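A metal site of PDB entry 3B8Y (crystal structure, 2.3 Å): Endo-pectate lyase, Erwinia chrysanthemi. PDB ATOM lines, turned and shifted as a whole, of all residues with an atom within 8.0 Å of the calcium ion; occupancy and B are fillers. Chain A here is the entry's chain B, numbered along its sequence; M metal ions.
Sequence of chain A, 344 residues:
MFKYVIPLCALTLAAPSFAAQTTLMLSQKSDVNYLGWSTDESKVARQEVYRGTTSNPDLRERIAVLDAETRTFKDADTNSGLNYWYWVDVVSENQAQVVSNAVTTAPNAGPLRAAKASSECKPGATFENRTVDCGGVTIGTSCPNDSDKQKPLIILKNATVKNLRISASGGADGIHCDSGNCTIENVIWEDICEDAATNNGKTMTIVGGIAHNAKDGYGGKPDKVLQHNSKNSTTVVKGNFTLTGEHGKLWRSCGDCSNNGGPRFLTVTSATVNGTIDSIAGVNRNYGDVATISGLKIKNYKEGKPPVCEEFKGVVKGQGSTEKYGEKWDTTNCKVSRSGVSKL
Of the 15 residues printed, 3 come within 4 Å of the calcium ion.
The nearest printed residue that does not touch the calcium ion is Ala 214 (4.02 Å).
The calcium ion is bound by the backbone carbonyl oxygen of Ile 192 (2.1 Å), the side-chain amide oxygen of Asn 213 (2.6 Å) and the side-chain carboxylate of Asp 191 (2.8 Å).
The calcium ion has three donor atoms within binding distance.
The backbone NH (N) of Ile 192 is in hydrogen-bond range of the backbone carbonyl oxygen (O) of His 212, 3.0 Å away.
OD2 of Asp 223 sits at hydrogen-bond distance from ND2 of Asn 213 (3.2 Å).
The backbone carbonyl oxygen of Asn 213 lies within hydrogen-bond range of the backbone NH of Glu 246.
OD1 of Asp 191 lies within hydrogen-bond range of N of Ala 214 (3.4 Å).
The side-chain sulfur of Cys 193 is disulfide-bonded to the side-chain sulfur of Cys 143, at 2.0 Å.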
ATOM      1  N   CYS A 143     -13.920   0.700 -10.708  1.00  0.00           N
ATOM      2  CA  CYS A 143     -15.050   0.054 -10.065  1.00  0.00           C
ATOM      3  C   CYS A 143     -15.129   0.394  -8.583  1.00  0.00           C
ATOM      4  O   CYS A 143     -14.666  -0.359  -7.730  1.00  0.00           O
ATOM      5  CB  CYS A 143     -14.987  -1.472 -10.256  1.00  0.00           C
ATOM      6  SG  CYS A 143     -16.338  -2.376  -9.434  1.00  0.00           S
ATOM      7  N   ALA A 168     -10.586  -7.004 -13.691  1.00  0.00           N
ATOM      8  CA  ALA A 168     -11.218  -7.177 -12.384  1.00  0.00           C
ATOM      9  C   ALA A 168     -11.363  -5.880 -11.577  1.00  0.00           C
ATOM     10  O   ALA A 168     -12.182  -5.805 -10.657  1.00  0.00           O
ATOM     11  CB  ALA A 168     -10.445  -8.216 -11.571  1.00  0.00           C
ATOM     12  N   GLY A 171     -14.224  -2.911 -13.978  1.00  0.00           N
ATOM     13  CA  GLY A 171     -15.533  -3.387 -14.411  1.00  0.00           C
ATOM     14  C   GLY A 171     -16.573  -2.355 -14.862  1.00  0.00           C
ATOM     15  O   GLY A 171     -17.104  -2.470 -15.973  1.00  0.00           O
ATOM     16  N   GLU A 190     -13.512 -10.741 -15.389  1.00  0.00           N
ATOM     17  CA  GLU A 190     -12.611 -11.157 -14.318  1.00  0.00           C
ATOM     18  C   GLU A 190     -13.269 -10.949 -12.962  1.00  0.00           C
ATOM     19  O   GLU A 190     -13.065 -11.731 -12.036  1.00  0.00           O
ATOM     20  CB  GLU A 190     -11.289 -10.394 -14.392  1.00  0.00           C
ATOM     21  CG  GLU A 190     -10.409 -10.803 -15.568  1.00  0.00           C
ATOM     22  CD  GLU A 190     -10.012 -12.270 -15.536  1.00  0.00           C
ATOM     23  OE1 GLU A 190     -10.068 -12.895 -14.447  1.00  0.00           O
ATOM     24  OE2 GLU A 190      -9.633 -12.809 -16.589  1.00  0.00           O
ATOM     25  N   ASP A 191     -14.093  -9.912 -12.885  1.00  0.00           N
ATOM     26  CA  ASP A 191     -14.831  -9.585 -11.673  1.00  0.00           C
ATOM     27  C   ASP A 191     -15.893  -8.551 -12.036  1.00  0.00           C
ATOM     28  O   ASP A 191     -15.574  -7.422 -12.379  1.00  0.00           O
ATOM     29  CB  ASP A 191     -13.900  -9.045 -10.588  1.00  0.00           C
ATOM     30  CG  ASP A 191     -14.574  -8.972  -9.233  1.00  0.00           C
ATOM     31  OD1 ASP A 191     -14.803 -10.037  -8.621  1.00  0.00           O
ATOM     32  OD2 ASP A 191     -14.873  -7.852  -8.793  1.00  0.00           O
ATOM     33  N   ILE A 192     -17.152  -8.982 -11.991  1.00  0.00           N
ATOM     34  CA  ILE A 192     -18.262  -8.105 -12.326  1.00  0.00           C
ATOM     35  C   ILE A 192     -18.377  -6.962 -11.331  1.00  0.00           C
ATOM     36  O   ILE A 192     -18.287  -7.156 -10.121  1.00  0.00           O
ATOM     37  CB  ILE A 192     -19.602  -8.883 -12.340  1.00  0.00           C
ATOM     38  CG1 ILE A 192     -19.543 -10.017 -13.361  1.00  0.00           C
ATOM     39  CG2 ILE A 192     -20.768  -7.945 -12.654  1.00  0.00           C
ATOM     40  CD1 ILE A 192     -20.764 -10.916 -13.361  1.00  0.00           C
ATOM     41  N   CYS A 193     -18.559  -5.744 -11.860  1.00  0.00           N
ATOM     42  CA  CYS A 193     -18.725  -4.579 -11.007  1.00  0.00           C
ATOM     43  C   CYS A 193     -20.211  -4.417 -10.681  1.00  0.00           C
ATOM     44  O   CYS A 193     -20.717  -5.108  -9.790  1.00  0.00           O
ATOM     45  CB  CYS A 193     -18.149  -3.325 -11.679  1.00  0.00           C
ATOM     46  SG  CYS A 193     -17.991  -1.923 -10.539  1.00  0.00           S
ATOM     47  N   GLU A 194     -20.908  -3.536 -11.393  1.00  0.00           N
ATOM     48  CA  GLU A 194     -22.348  -3.329 -11.172  1.00  0.00           C
ATOM     49  C   GLU A 194     -23.139  -4.504 -11.763  1.00  0.00           C
ATOM     50  O   GLU A 194     -23.866  -5.202 -11.053  1.00  0.00           O
ATOM     51  CB  GLU A 194     -22.810  -2.000 -11.776  1.00  0.00           C
ATOM     52  CG  GLU A 194     -22.384  -0.739 -10.994  1.00  0.00           C
ATOM     53  CD  GLU A 194     -23.270  -0.454  -9.779  1.00  0.00           C
ATOM     54  OE1 GLU A 194     -24.209  -1.237  -9.490  1.00  0.00           O
ATOM     55  OE2 GLU A 194     -23.035   0.585  -9.110  1.00  0.00           O
ATOM     56  N   ASP A 195     -23.009  -4.683 -13.080  1.00  0.00           N
ATOM     57  CA  ASP A 195     -23.648  -5.783 -13.780  1.00  0.00           C
ATOM     58  C   ASP A 195     -22.885  -6.113 -15.057  1.00  0.00           C
ATOM     59  O   ASP A 195     -22.426  -5.213 -15.762  1.00  0.00           O
ATOM     60  CB  ASP A 195     -25.147  -5.534 -14.042  1.00  0.00           C
ATOM     61  CG  ASP A 195     -25.427  -4.182 -14.653  1.00  0.00           C
ATOM     62  OD1 ASP A 195     -26.143  -3.390 -14.019  1.00  0.00           O
ATOM     63  OD2 ASP A 195     -24.942  -3.939 -15.790  1.00  0.00           O
ATOM     64  N   HIS A 212     -16.916 -14.100 -13.710  1.00  0.00           N
ATOM     65  CA  HIS A 212     -16.541 -14.291 -12.335  1.00  0.00           C
ATOM     66  C   HIS A 212     -16.946 -13.103 -11.471  1.00  0.00           C
ATOM     67  O   HIS A 212     -16.948 -11.952 -11.917  1.00  0.00           O
ATOM     68  CB  HIS A 212     -15.029 -14.506 -12.212  1.00  0.00           C
ATOM     69  CG  HIS A 212     -14.545 -14.589 -10.800  1.00  0.00           C
ATOM     70  ND1 HIS A 212     -14.715 -15.711 -10.017  1.00  0.00           N
ATOM     71  CD2 HIS A 212     -13.934 -13.662 -10.021  1.00  0.00           C
ATOM     72  CE1 HIS A 212     -14.233 -15.477  -8.810  1.00  0.00           C
ATOM     73  NE2 HIS A 212     -13.753 -14.241  -8.785  1.00  0.00           N
ATOM     74  N   ASN A 213     -17.284 -13.400 -10.217  1.00  0.00           N
ATOM     75  CA  ASN A 213     -17.635 -12.368  -9.254  1.00  0.00           C
ATOM     76  C   ASN A 213     -17.354 -12.885  -7.850  1.00  0.00           C
ATOM     77  O   ASN A 213     -17.436 -14.086  -7.587  1.00  0.00           O
ATOM     78  CB  ASN A 213     -19.111 -11.979  -9.376  1.00  0.00           C
ATOM     79  CG  ASN A 213     -19.434 -10.729  -8.594  1.00  0.00           C
ATOM     80  OD1 ASN A 213     -19.328  -9.617  -9.111  1.00  0.00           O
ATOM     81  ND2 ASN A 213     -19.794 -10.897  -7.336  1.00  0.00           N
ATOM     82  N   ALA A 214     -17.017 -11.962  -6.954  1.00  0.00           N
ATOM     83  CA  ALA A 214     -16.703 -12.287  -5.574  1.00  0.00           C
ATOM     84  C   ALA A 214     -17.305 -11.277  -4.602  1.00  0.00           C
ATOM     85  O   ALA A 214     -17.380 -10.081  -4.913  1.00  0.00           O
ATOM     86  CB  ALA A 214     -15.187 -12.367  -5.373  1.00  0.00           C
ATOM     87  N   ASP A 223     -25.304  -9.328  -6.211  1.00  0.00           N
ATOM     88  CA  ASP A 223     -24.867  -8.723  -7.468  1.00  0.00           C
ATOM     89  C   ASP A 223     -25.695  -9.267  -8.631  1.00  0.00           C
ATOM     90  O   ASP A 223     -26.234 -10.379  -8.558  1.00  0.00           O
ATOM     91  CB  ASP A 223     -23.384  -9.009  -7.733  1.00  0.00           C
ATOM     92  CG  ASP A 223     -22.621  -9.406  -6.481  1.00  0.00           C
ATOM     93  OD1 ASP A 223     -21.894  -8.553  -5.923  1.00  0.00           O
ATOM     94  OD2 ASP A 223     -22.740 -10.583  -6.065  1.00  0.00           O
ATOM     95  N   GLU A 246     -19.230 -16.077  -6.588  1.00  0.00           N
ATOM     96  CA  GLU A 246     -20.536 -15.820  -5.964  1.00  0.00           C
ATOM     97  C   GLU A 246     -21.342 -14.890  -6.848  1.00  0.00           C
ATOM     98  O   GLU A 246     -20.822 -13.917  -7.384  1.00  0.00           O
ATOM     99  CB  GLU A 246     -20.354 -15.188  -4.583  1.00  0.00           C
ATOM    100  CG  GLU A 246     -19.439 -15.953  -3.625  1.00  0.00           C
ATOM    101  CD  GLU A 246     -17.979 -15.571  -3.777  1.00  0.00           C
ATOM    102  OE1 GLU A 246     -17.588 -14.474  -3.305  1.00  0.00           O
ATOM    103  OE2 GLU A 246     -17.202 -16.370  -4.351  1.00  0.00           O
ATOM    104  N   HIS A 247     -22.621 -15.209  -6.998  1.00  0.00           N
ATOM    105  CA  HIS A 247     -23.506 -14.398  -7.817  1.00  0.00           C
ATOM    106  C   HIS A 247     -24.890 -14.282  -7.206  1.00  0.00           C
ATOM    107  O   HIS A 247     -25.344 -15.189  -6.515  1.00  0.00           O
ATOM    108  CB  HIS A 247     -23.635 -15.013  -9.216  1.00  0.00           C
ATOM    109  CG  HIS A 247     -22.361 -14.994 -10.012  1.00  0.00           C
ATOM    110  ND1 HIS A 247     -21.919 -13.882 -10.682  1.00  0.00           N
ATOM    111  CD2 HIS A 247     -21.456 -15.969 -10.260  1.00  0.00           C
ATOM    112  CE1 HIS A 247     -20.795 -14.157 -11.308  1.00  0.00           C
ATOM    113  NE2 HIS A 247     -20.492 -15.421 -11.077  1.00  0.00           N
HETATM  114 CA    CA M   1     -17.592  -7.932  -8.302  1.00  0.00          CA
